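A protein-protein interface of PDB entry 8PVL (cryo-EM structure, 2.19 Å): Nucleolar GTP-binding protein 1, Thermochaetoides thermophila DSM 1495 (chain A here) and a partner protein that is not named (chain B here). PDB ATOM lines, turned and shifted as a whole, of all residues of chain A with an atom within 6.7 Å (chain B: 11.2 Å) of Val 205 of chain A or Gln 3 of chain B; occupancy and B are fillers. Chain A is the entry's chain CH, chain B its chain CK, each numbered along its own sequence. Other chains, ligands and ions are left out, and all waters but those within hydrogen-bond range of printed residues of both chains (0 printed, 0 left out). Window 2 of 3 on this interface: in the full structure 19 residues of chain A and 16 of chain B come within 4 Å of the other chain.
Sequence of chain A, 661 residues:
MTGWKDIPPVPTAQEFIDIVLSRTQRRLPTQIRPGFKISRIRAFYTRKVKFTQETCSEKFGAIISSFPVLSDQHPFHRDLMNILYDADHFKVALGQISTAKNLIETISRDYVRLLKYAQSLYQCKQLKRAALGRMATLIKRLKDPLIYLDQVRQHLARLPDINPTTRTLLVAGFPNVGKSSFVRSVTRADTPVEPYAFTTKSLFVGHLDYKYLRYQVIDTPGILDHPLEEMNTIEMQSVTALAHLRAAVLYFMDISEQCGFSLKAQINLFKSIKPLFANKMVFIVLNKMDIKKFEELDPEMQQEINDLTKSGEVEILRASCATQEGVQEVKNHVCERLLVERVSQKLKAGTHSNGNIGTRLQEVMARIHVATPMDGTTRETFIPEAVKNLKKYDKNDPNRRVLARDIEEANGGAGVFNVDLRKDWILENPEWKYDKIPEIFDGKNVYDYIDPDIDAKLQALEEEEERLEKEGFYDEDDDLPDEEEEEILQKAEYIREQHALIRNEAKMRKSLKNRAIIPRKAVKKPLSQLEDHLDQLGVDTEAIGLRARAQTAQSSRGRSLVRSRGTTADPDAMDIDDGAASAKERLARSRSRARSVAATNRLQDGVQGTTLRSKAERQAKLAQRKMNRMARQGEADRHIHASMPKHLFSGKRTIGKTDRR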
ATOM      1  N   ARG A 158     -21.603 -20.893  -0.625  1.00  0.00           N
ATOM      2  CA  ARG A 158     -22.551 -21.756   0.068  1.00  0.00           C
ATOM      3  C   ARG A 158     -23.344 -21.044   1.162  1.00  0.00           C
ATOM      4  O   ARG A 158     -24.128 -21.697   1.856  1.00  0.00           O
ATOM      5  CB  ARG A 158     -21.829 -22.969   0.651  1.00  0.00           C
ATOM      6  CG  ARG A 158     -21.071 -23.766  -0.388  1.00  0.00           C
ATOM      7  CD  ARG A 158     -20.692 -25.127   0.136  1.00  0.00           C
ATOM      8  NE  ARG A 158     -20.037 -25.045   1.434  1.00  0.00           N
ATOM      9  CZ  ARG A 158     -18.734 -24.879   1.605  1.00  0.00           C
ATOM     10  NH1 ARG A 158     -17.910 -24.780   0.576  1.00  0.00           N
ATOM     11  NH2 ARG A 158     -18.246 -24.809   2.838  1.00  0.00           N
ATOM     12  N   LEU A 159     -23.160 -19.737   1.336  1.00  0.00           N
ATOM     13  CA  LEU A 159     -23.915 -18.997   2.341  1.00  0.00           C
ATOM     14  C   LEU A 159     -25.399 -18.944   1.981  1.00  0.00           C
ATOM     15  O   LEU A 159     -25.750 -18.824   0.801  1.00  0.00           O
ATOM     16  CB  LEU A 159     -23.382 -17.570   2.477  1.00  0.00           C
ATOM     17  CG  LEU A 159     -22.425 -17.209   3.614  1.00  0.00           C
ATOM     18  CD1 LEU A 159     -22.327 -15.700   3.745  1.00  0.00           C
ATOM     19  CD2 LEU A 159     -22.860 -17.824   4.928  1.00  0.00           C
ATOM     20  N   PRO A 160     -26.294 -19.029   2.964  1.00  0.00           N
ATOM     21  CA  PRO A 160     -27.722 -18.838   2.685  1.00  0.00           C
ATOM     22  C   PRO A 160     -28.056 -17.391   2.356  1.00  0.00           C
ATOM     23  O   PRO A 160     -27.379 -16.456   2.787  1.00  0.00           O
ATOM     24  CB  PRO A 160     -28.398 -19.271   3.991  1.00  0.00           C
ATOM     25  CG  PRO A 160     -27.348 -19.159   5.027  1.00  0.00           C
ATOM     26  CD  PRO A 160     -26.062 -19.485   4.344  1.00  0.00           C
ATOM     27  N   ASP A 161     -29.129 -17.218   1.589  1.00  0.00           N
ATOM     28  CA  ASP A 161     -29.601 -15.899   1.183  1.00  0.00           C
ATOM     29  C   ASP A 161     -30.651 -15.426   2.182  1.00  0.00           C
ATOM     30  O   ASP A 161     -31.740 -16.002   2.268  1.00  0.00           O
ATOM     31  CB  ASP A 161     -30.170 -15.944  -0.232  1.00  0.00           C
ATOM     32  CG  ASP A 161     -30.374 -14.564  -0.828  1.00  0.00           C
ATOM     33  OD1 ASP A 161     -29.920 -13.573  -0.222  1.00  0.00           O
ATOM     34  OD2 ASP A 161     -30.996 -14.471  -1.906  1.00  0.00           O
ATOM     35  N   ILE A 162     -30.327 -14.379   2.932  1.00  0.00           N
ATOM     36  CA  ILE A 162     -31.212 -13.829   3.951  1.00  0.00           C
ATOM     37  C   ILE A 162     -31.518 -12.387   3.584  1.00  0.00           C
ATOM     38  O   ILE A 162     -30.601 -11.574   3.418  1.00  0.00           O
ATOM     39  CB  ILE A 162     -30.590 -13.921   5.354  1.00  0.00           C
ATOM     40  CG1 ILE A 162     -30.538 -15.378   5.816  1.00  0.00           C
ATOM     41  CG2 ILE A 162     -31.367 -13.068   6.341  1.00  0.00           C
ATOM     42  CD1 ILE A 162     -29.887 -15.568   7.163  1.00  0.00           C
ATOM     43  N   ASN A 163     -32.803 -12.073   3.450  1.00  0.00           N
ATOM     44  CA  ASN A 163     -33.235 -10.709   3.183  1.00  0.00           C
ATOM     45  C   ASN A 163     -33.454  -9.994   4.508  1.00  0.00           C
ATOM     46  O   ASN A 163     -34.334 -10.399   5.278  1.00  0.00           O
ATOM     47  CB  ASN A 163     -34.514 -10.708   2.362  1.00  0.00           C
ATOM     48  CG  ASN A 163     -34.853  -9.343   1.786  1.00  0.00           C
ATOM     49  OD1 ASN A 163     -34.176  -8.351   2.046  1.00  0.00           O
ATOM     50  ND2 ASN A 163     -35.914  -9.292   0.991  1.00  0.00           N
ATOM     51  N   VAL A 183     -38.171 -25.525  12.861  1.00  0.00           N
ATOM     52  CA  VAL A 183     -37.928 -24.993  11.522  1.00  0.00           C
ATOM     53  C   VAL A 183     -38.173 -26.065  10.462  1.00  0.00           C
ATOM     54  O   VAL A 183     -38.727 -25.780   9.393  1.00  0.00           O
ATOM     55  CB  VAL A 183     -36.511 -24.392  11.438  1.00  0.00           C
ATOM     56  CG1 VAL A 183     -36.197 -23.921  10.029  1.00  0.00           C
ATOM     57  CG2 VAL A 183     -36.398 -23.223  12.394  1.00  0.00           C
ATOM     58  N   THR A 187     -41.069 -25.368   7.728  1.00  0.00           N
ATOM     59  CA  THR A 187     -40.480 -25.003   6.444  1.00  0.00           C
ATOM     60  C   THR A 187     -40.018 -26.256   5.710  1.00  0.00           C
ATOM     61  O   THR A 187     -40.227 -27.386   6.158  1.00  0.00           O
ATOM     62  CB  THR A 187     -39.302 -24.030   6.608  1.00  0.00           C
ATOM     63  OG1 THR A 187     -38.294 -24.625   7.432  1.00  0.00           O
ATOM     64  CG2 THR A 187     -39.754 -22.714   7.222  1.00  0.00           C
ATOM     65  N   ARG A 188     -39.387 -26.038   4.558  1.00  0.00           N
ATOM     66  CA  ARG A 188     -38.809 -27.099   3.746  1.00  0.00           C
ATOM     67  C   ARG A 188     -37.294 -27.185   3.882  1.00  0.00           C
ATOM     68  O   ARG A 188     -36.666 -27.970   3.166  1.00  0.00           O
ATOM     69  CB  ARG A 188     -39.185 -26.893   2.274  1.00  0.00           C
ATOM     70  CG  ARG A 188     -39.526 -28.167   1.524  1.00  0.00           C
ATOM     71  CD  ARG A 188     -40.014 -27.865   0.114  1.00  0.00           C
ATOM     72  NE  ARG A 188     -38.932 -27.456  -0.773  1.00  0.00           N
ATOM     73  CZ  ARG A 188     -38.096 -28.292  -1.377  1.00  0.00           C
ATOM     74  NH1 ARG A 188     -38.189 -29.602  -1.211  1.00  0.00           N
ATOM     75  NH2 ARG A 188     -37.146 -27.801  -2.167  1.00  0.00           N
ATOM     76  N   ALA A 189     -36.698 -26.401   4.777  1.00  0.00           N
ATOM     77  CA  ALA A 189     -35.248 -26.364   4.910  1.00  0.00           C
ATOM     78  C   ALA A 189     -34.719 -27.652   5.526  1.00  0.00           C
ATOM     79  O   ALA A 189     -35.326 -28.223   6.436  1.00  0.00           O
ATOM     80  CB  ALA A 189     -34.822 -25.167   5.758  1.00  0.00           C
ATOM     81  N   ASP A 190     -33.578 -28.109   5.020  1.00  0.00           N
ATOM     82  CA  ASP A 190     -32.948 -29.336   5.503  1.00  0.00           C
ATOM     83  C   ASP A 190     -31.890 -28.992   6.550  1.00  0.00           C
ATOM     84  O   ASP A 190     -30.684 -29.027   6.309  1.00  0.00           O
ATOM     85  CB  ASP A 190     -32.357 -30.120   4.335  1.00  0.00           C
ATOM     86  CG  ASP A 190     -31.851 -31.488   4.746  1.00  0.00           C
ATOM     87  OD1 ASP A 190     -32.290 -31.998   5.797  1.00  0.00           O
ATOM     88  OD2 ASP A 190     -31.010 -32.053   4.017  1.00  0.00           O
ATOM     89  N   THR A 191     -32.377 -28.640   7.739  1.00  0.00           N
ATOM     90  CA  THR A 191     -31.506 -28.405   8.880  1.00  0.00           C
ATOM     91  C   THR A 191     -31.506 -29.637   9.771  1.00  0.00           C
ATOM     92  O   THR A 191     -32.587 -30.106  10.161  1.00  0.00           O
ATOM     93  CB  THR A 191     -31.944 -27.166   9.659  1.00  0.00           C
ATOM     94  OG1 THR A 191     -31.360 -27.178  10.967  1.00  0.00           O
ATOM     95  CG2 THR A 191     -33.469 -27.059   9.755  1.00  0.00           C
ATOM     96  N   LEU A 203     -26.189 -20.433  10.227  1.00  0.00           N
ATOM     97  CA  LEU A 203     -27.555 -19.979  10.025  1.00  0.00           C
ATOM     98  C   LEU A 203     -28.213 -20.768   8.900  1.00  0.00           C
ATOM     99  O   LEU A 203     -27.629 -20.962   7.832  1.00  0.00           O
ATOM    100  CB  LEU A 203     -27.582 -18.486   9.704  1.00  0.00           C
ATOM    101  CG  LEU A 203     -27.100 -17.544  10.806  1.00  0.00           C
ATOM    102  CD1 LEU A 203     -27.005 -16.122  10.287  1.00  0.00           C
ATOM    103  CD2 LEU A 203     -28.020 -17.616  12.008  1.00  0.00           C
ATOM    104  N   PHE A 204     -29.431 -21.240   9.152  1.00  0.00           N
ATOM    105  CA  PHE A 204     -30.245 -21.889   8.138  1.00  0.00           C
ATOM    106  C   PHE A 204     -31.488 -21.044   7.903  1.00  0.00           C
ATOM    107  O   PHE A 204     -31.988 -20.394   8.821  1.00  0.00           O
ATOM    108  CB  PHE A 204     -30.657 -23.305   8.560  1.00  0.00           C
ATOM    109  CG  PHE A 204     -29.555 -24.322   8.463  1.00  0.00           C
ATOM    110  CD1 PHE A 204     -28.598 -24.426   9.460  1.00  0.00           C
ATOM    111  CD2 PHE A 204     -29.488 -25.189   7.385  1.00  0.00           C
ATOM    112  CE1 PHE A 204     -27.587 -25.365   9.377  1.00  0.00           C
ATOM    113  CE2 PHE A 204     -28.480 -26.132   7.295  1.00  0.00           C
ATOM    114  CZ  PHE A 204     -27.530 -26.221   8.294  1.00  0.00           C
ATOM    115  N   VAL A 205     -31.985 -21.037   6.671  1.00  0.00           N
ATOM    116  CA  VAL A 205     -33.199 -20.298   6.346  1.00  0.00           C
ATOM    117  C   VAL A 205     -34.154 -21.220   5.598  1.00  0.00           C
ATOM    118  O   VAL A 205     -33.750 -21.936   4.677  1.00  0.00           O
ATOM    119  CB  VAL A 205     -32.896 -19.014   5.540  1.00  0.00           C
ATOM    120  CG1 VAL A 205     -32.007 -19.299   4.354  1.00  0.00           C
ATOM    121  CG2 VAL A 205     -34.180 -18.321   5.096  1.00  0.00           C
ATOM    122  N   GLY A 206     -35.410 -21.243   6.043  1.00  0.00           N
ATOM    123  CA  GLY A 206     -36.496 -21.839   5.303  1.00  0.00           C
ATOM    124  C   GLY A 206     -37.535 -20.781   4.974  1.00  0.00           C
ATOM    125  O   GLY A 206     -37.420 -19.620   5.369  1.00  0.00           O
ATOM    126  N   HIS A 207     -38.562 -21.208   4.249  1.00  0.00           N
ATOM    127  CA  HIS A 207     -39.607 -20.289   3.830  1.00  0.00           C
ATOM    128  C   HIS A 207     -40.970 -20.924   4.053  1.00  0.00           C
ATOM    129  O   HIS A 207     -41.117 -22.148   4.065  1.00  0.00           O
ATOM    130  CB  HIS A 207     -39.440 -19.882   2.361  1.00  0.00           C
ATOM    131  CG  HIS A 207     -38.220 -19.056   2.098  1.00  0.00           C
ATOM    132  ND1 HIS A 207     -36.954 -19.596   2.035  1.00  0.00           N
ATOM    133  CD2 HIS A 207     -38.074 -17.728   1.881  1.00  0.00           C
ATOM    134  CE1 HIS A 207     -36.080 -18.636   1.792  1.00  0.00           C
ATOM    135  NE2 HIS A 207     -36.734 -17.493   1.692  1.00  0.00           N
ATOM    136  N   GLN A 216     -39.824 -15.702   5.752  1.00  0.00           N
ATOM    137  CA  GLN A 216     -38.602 -16.478   5.898  1.00  0.00           C
ATOM    138  C   GLN A 216     -38.355 -16.756   7.375  1.00  0.00           C
ATOM    139  O   GLN A 216     -38.660 -15.925   8.233  1.00  0.00           O
ATOM    140  CB  GLN A 216     -37.401 -15.772   5.250  1.00  0.00           C
ATOM    141  CG  GLN A 216     -36.847 -14.568   5.983  1.00  0.00           C
ATOM    142  CD  GLN A 216     -35.652 -13.961   5.276  1.00  0.00           C
ATOM    143  OE1 GLN A 216     -35.297 -14.370   4.172  1.00  0.00           O
ATOM    144  NE2 GLN A 216     -35.026 -12.977   5.909  1.00  0.00           N
ATOM    145  N   VAL A 217     -37.859 -17.955   7.666  1.00  0.00           N
ATOM    146  CA  VAL A 217     -37.632 -18.426   9.026  1.00  0.00           C
ATOM    147  C   VAL A 217     -36.158 -18.773   9.160  1.00  0.00           C
ATOM    148  O   VAL A 217     -35.623 -19.542   8.355  1.00  0.00           O
ATOM    149  CB  VAL A 217     -38.509 -19.647   9.357  1.00  0.00           C
ATOM    150  CG1 VAL A 217     -38.259 -20.119  10.777  1.00  0.00           C
ATOM    151  CG2 VAL A 217     -39.971 -19.314   9.156  1.00  0.00           C
ATOM    152  N   ILE A 218     -35.507 -18.218  10.175  1.00  0.00           N
ATOM    153  CA  ILE A 218     -34.067 -18.358  10.344  1.00  0.00           C
ATOM    154  C   ILE A 218     -33.800 -19.189  11.592  1.00  0.00           C
ATOM    155  O   ILE A 218     -34.077 -18.756  12.720  1.00  0.00           O
ATOM    156  CB  ILE A 218     -33.371 -16.995  10.414  1.00  0.00           C
ATOM    157  CG1 ILE A 218     -33.613 -16.235   9.112  1.00  0.00           C
ATOM    158  CG2 ILE A 218     -31.883 -17.174  10.650  1.00  0.00           C
ATOM    159  CD1 ILE A 218     -33.106 -14.833   9.126  1.00  0.00           C
ATOM    160  N   ASP A 219     -33.257 -20.383  11.371  1.00  0.00           N
ATOM    161  CA  ASP A 219     -32.736 -21.244  12.420  1.00  0.00           C
ATOM    162  C   ASP A 219     -31.299 -20.855  12.735  1.00  0.00           C
ATOM    163  O   ASP A 219     -30.483 -20.648  11.831  1.00  0.00           O
ATOM    164  CB  ASP A 219     -32.792 -22.709  11.984  1.00  0.00           C
ATOM    165  CG  ASP A 219     -32.415 -23.668  13.096  1.00  0.00           C
ATOM    166  OD1 ASP A 219     -32.435 -23.260  14.276  1.00  0.00           O
ATOM    167  OD2 ASP A 219     -32.102 -24.836  12.789  1.00  0.00           O
ATOM    168  N   PRO B   2     -29.699 -24.757  -2.025  1.00  0.00           N
ATOM    169  CA  PRO B   2     -29.022 -25.438  -0.924  1.00  0.00           C
ATOM    170  C   PRO B   2     -28.139 -24.474  -0.146  1.00  0.00           C
ATOM    171  O   PRO B   2     -27.800 -23.404  -0.648  1.00  0.00           O
ATOM    172  CB  PRO B   2     -28.203 -26.501  -1.641  1.00  0.00           C
ATOM    173  CG  PRO B   2     -27.844 -25.865  -2.917  1.00  0.00           C
ATOM    174  CD  PRO B   2     -28.965 -24.924  -3.287  1.00  0.00           C
ATOM    175  N   GLN B   3     -27.786 -24.850   1.078  1.00  0.00           N
ATOM    176  CA  GLN B   3     -27.047 -23.965   1.962  1.00  0.00           C
ATOM    177  C   GLN B   3     -26.082 -24.787   2.800  1.00  0.00           C
ATOM    178  O   GLN B   3     -26.322 -25.969   3.062  1.00  0.00           O
ATOM    179  CB  GLN B   3     -27.998 -23.172   2.862  1.00  0.00           C
ATOM    180  CG  GLN B   3     -29.096 -24.028   3.472  1.00  0.00           C
ATOM    181  CD  GLN B   3     -30.238 -23.211   4.031  1.00  0.00           C
ATOM    182  OE1 GLN B   3     -30.061 -22.061   4.421  1.00  0.00           O
ATOM    183  NE2 GLN B   3     -31.421 -23.804   4.074  1.00  0.00           N
ATOM    184  N   ASN B   4     -24.998 -24.140   3.214  1.00  0.00           N
ATOM    185  CA  ASN B   4     -23.955 -24.685   4.104  1.00  0.00           C
ATOM    186  C   ASN B   4     -23.326 -25.902   3.412  1.00  0.00           C
ATOM    187  O   ASN B   4     -23.061 -25.850   2.204  1.00  0.00           O
ATOM    188  CB  ASN B   4     -24.541 -24.935   5.477  1.00  0.00           C
ATOM    189  CG  ASN B   4     -25.100 -23.673   6.100  1.00  0.00           C
ATOM    190  OD1 ASN B   4     -24.418 -22.653   6.175  1.00  0.00           O
ATOM    191  ND2 ASN B   4     -26.348 -23.730   6.537  1.00  0.00           N
ATOM    192  N   GLU B   5     -23.081 -26.999   4.122  1.00  0.00           N
ATOM    193  CA  GLU B   5     -22.315 -28.114   3.568  1.00  0.00           C
ATOM    194  C   GLU B   5     -23.253 -29.165   2.972  1.00  0.00           C
ATOM    195  O   GLU B   5     -23.379 -30.293   3.458  1.00  0.00           O
ATOM    196  CB  GLU B   5     -21.410 -28.714   4.638  1.00  0.00           C
ATOM    197  CG  GLU B   5     -20.077 -28.009   4.784  1.00  0.00           C
ATOM    198  CD  GLU B   5     -20.193 -26.702   5.538  1.00  0.00           C
ATOM    199  OE1 GLU B   5     -20.996 -26.634   6.492  1.00  0.00           O
ATOM    200  OE2 GLU B   5     -19.485 -25.740   5.175  1.00  0.00           O
ATOM    201  N   TYR B   6     -23.895 -28.779   1.867  1.00  0.00           N
ATOM    202  CA  TYR B   6     -24.958 -29.611   1.313  1.00  0.00           C
ATOM    203  C   TYR B   6     -24.433 -30.831   0.562  1.00  0.00           C
ATOM    204  O   TYR B   6     -25.102 -31.867   0.553  1.00  0.00           O
ATOM    205  CB  TYR B   6     -25.876 -28.778   0.414  1.00  0.00           C
ATOM    206  CG  TYR B   6     -25.190 -27.920  -0.622  1.00  0.00           C
ATOM    207  CD1 TYR B   6     -24.880 -28.429  -1.877  1.00  0.00           C
ATOM    208  CD2 TYR B   6     -24.884 -26.591  -0.359  1.00  0.00           C
ATOM    209  CE1 TYR B   6     -24.267 -27.643  -2.833  1.00  0.00           C
ATOM    210  CE2 TYR B   6     -24.271 -25.799  -1.308  1.00  0.00           C
ATOM    211  CZ  TYR B   6     -23.967 -26.329  -2.542  1.00  0.00           C
ATOM    212  OH  TYR B   6     -23.356 -25.545  -3.490  1.00  0.00           O
ATOM    213  N   ILE B   7     -23.250 -30.755  -0.051  1.00  0.00           N
ATOM    214  CA  ILE B   7     -22.689 -31.944  -0.694  1.00  0.00           C
ATOM    215  C   ILE B   7     -22.258 -32.965   0.354  1.00  0.00           C
ATOM    216  O   ILE B   7     -22.466 -34.173   0.184  1.00  0.00           O
ATOM    217  CB  ILE B   7     -21.539 -31.552  -1.642  1.00  0.00           C
ATOM    218  CG1 ILE B   7     -22.099 -30.914  -2.915  1.00  0.00           C
ATOM    219  CG2 ILE B   7     -20.672 -32.747  -2.010  1.00  0.00           C
ATOM    220  CD1 ILE B   7     -23.084 -31.790  -3.655  1.00  0.00           C
ATOM    221  N   GLU B   8     -21.679 -32.499   1.465  1.00  0.00           N
ATOM    222  CA  GLU B   8     -21.354 -33.401   2.568  1.00  0.00           C
ATOM    223  C   GLU B   8     -22.614 -34.010   3.174  1.00  0.00           C
ATOM    224  O   GLU B   8     -22.631 -35.199   3.520  1.00  0.00           O
ATOM    225  CB  GLU B   8     -20.548 -32.659   3.634  1.00  0.00           C
ATOM    226  CG  GLU B   8     -19.122 -32.343   3.224  1.00  0.00           C
ATOM    227  CD  GLU B   8     -18.443 -31.373   4.170  1.00  0.00           C
ATOM    228  OE1 GLU B   8     -18.861 -31.295   5.344  1.00  0.00           O
ATOM    229  OE2 GLU B   8     -17.496 -30.684   3.739  1.00  0.00           O
ATOM    230  N   ARG B   9     -23.682 -33.217   3.298  1.00  0.00           N
ATOM    231  CA  ARG B   9     -24.942 -33.753   3.809  1.00  0.00           C
ATOM    232  C   ARG B   9     -25.549 -34.774   2.848  1.00  0.00           C
ATOM    233  O   ARG B   9     -26.110 -35.787   3.284  1.00  0.00           O
ATOM    234  CB  ARG B   9     -25.919 -32.608   4.088  1.00  0.00           C
ATOM    235  CG  ARG B   9     -27.302 -33.064   4.518  1.00  0.00           C
ATOM    236  CD  ARG B   9     -27.805 -32.284   5.715  1.00  0.00           C
ATOM    237  NE  ARG B   9     -29.129 -32.734   6.127  1.00  0.00           N
ATOM    238  CZ  ARG B   9     -29.353 -33.698   7.008  1.00  0.00           C
ATOM    239  NH1 ARG B   9     -28.359 -34.332   7.607  1.00  0.00           N
ATOM    240  NH2 ARG B   9     -30.607 -34.037   7.295  1.00  0.00           N
ATOM    241  N   HIS B  10     -25.434 -34.536   1.538  1.00  0.00           N
ATOM    242  CA  HIS B  10     -25.922 -35.498   0.555  1.00  0.00           C
ATOM    243  C   HIS B  10     -25.108 -36.786   0.584  1.00  0.00           C
ATOM    244  O   HIS B  10     -25.657 -37.876   0.396  1.00  0.00           O
ATOM    245  CB  HIS B  10     -25.896 -34.880  -0.842  1.00  0.00           C
ATOM    246  CG  HIS B  10     -26.385 -35.800  -1.915  1.00  0.00           C
ATOM    247  ND1 HIS B  10     -27.715 -35.907  -2.256  1.00  0.00           N
ATOM    248  CD2 HIS B  10     -25.720 -36.663  -2.718  1.00  0.00           C
ATOM    249  CE1 HIS B  10     -27.848 -36.793  -3.226  1.00  0.00           C
ATOM    250  NE2 HIS B  10     -26.653 -37.267  -3.524  1.00  0.00           N
ATOM    251  N   LEU B  13     -26.399 -38.654   3.640  1.00  0.00           N
ATOM    252  CA  LEU B  13     -27.743 -39.209   3.524  1.00  0.00           C
ATOM    253  C   LEU B  13     -27.859 -40.275   2.440  1.00  0.00           C
ATOM    254  O   LEU B  13     -28.677 -41.191   2.575  1.00  0.00           O
ATOM    255  CB  LEU B  13     -28.753 -38.093   3.257  1.00  0.00           C
ATOM    256  CG  LEU B  13     -29.047 -37.154   4.427  1.00  0.00           C
ATOM    257  CD1 LEU B  13     -30.059 -36.095   4.026  1.00  0.00           C
ATOM    258  CD2 LEU B  13     -29.535 -37.938   5.630  1.00  0.00           C
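The backbone carbonyl oxygen of Phe 204 of chain A sits at hydrogen-bond distance from the backbone NH of Asp 219 of chain A (2.8 Å).
O of Arg 158 of chain A lies within hydrogen-bond range of N of Asn 4 of chain B.
NH2 of Arg 158 of chain A is in salt-bridge range of OE2 of Glu 5 of chain B, 2.8 Å away.
OD2 of Asp 190 of chain A is in salt-bridge range of NE of Arg 9 of chain B, at 2.9 Å.
The backbone carbonyl oxygen of Leu 203 of chain A sits at hydrogen-bond distance from the side-chain amide nitrogen of Asn 4 of chain B, at 3.3 Å.
O of Val 205 of chain A is in hydrogen-bond range of NE2 of Gln 3 of chain B (3.0 Å).
Printed residues of chain B within 4 Å of Arg 158 of chain A: Gln 3, Asn 4, Glu 5 and Tyr 6.
Printed residues of chain B within 4 Å of Pro 160 of chain A: Gln 3.
Asn 163 of chain A touches none of the printed residues of chain B.
Printed residues of chain B within 4 Å of Asp 190 of chain A: Arg 9.
Phe 204 of chain A touches two residues of chain B.
Val 205 of chain A touches just one residue of chain B: Gln 3 (3.0 Å).
No residue of chain B comes within 4 Å of Gly 206 of chain A.
Gln 216 of chain A touches none of the printed residues of chain B.
No residue of chain B comes within 4 Å of Val 217 of chain A.
Gln 3 of chain B touches just these residues of chain A: Arg 158 (3.7 Å), Pro 160 (3.3 Å), Phe 204 (3.7 Å) and Val 205 (3.0 Å).
Printed residues of chain A within 4 Å of Asn 4 of chain B: Arg 158, Leu 203 and Phe 204.
Leu 13 of chain B touches none of the printed residues of chain A.
The nearest residue of chain B that does not touch Val 205 of chain A is Asn 4 of chain B (6.2 Å).
O of Arg 158 of chain A touches CA of Gln 3 of chain B (3.7 Å).
CE2 of Tyr 6 of chain B touches CG of Arg 158 of chain A, 3.9 Å away.
OE1 of Gln 3 of chain B touches CB of Pro 160 of chain A, at 3.3 Å.
Phe 204 of chain A touches Gln 3 of chain B (CA to OE1, 3.7 Å).
Phe 204 of chain A touches Asn 4 of chain B.
Along chain A the printed residues that touch a printed residue of chain B span positions 158 to 205.
Of the 10 printed residues of chain B, 5 touch a printed residue of chain A.
Printed residues of chain B that touch a printed residue of chain A: Gln 3, Asn 4, Glu 5, Tyr 6 and Arg 9.
Among the printed residues, Asp or Glu carboxylates within 4 Å of a Lys or Arg side-chain nitrogen of the other chain: Arg 158 of chain A with Glu 5 of chain B (2.8 Å) and Asp 190 of chain A with Arg 9 of chain B (2.9 Å).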
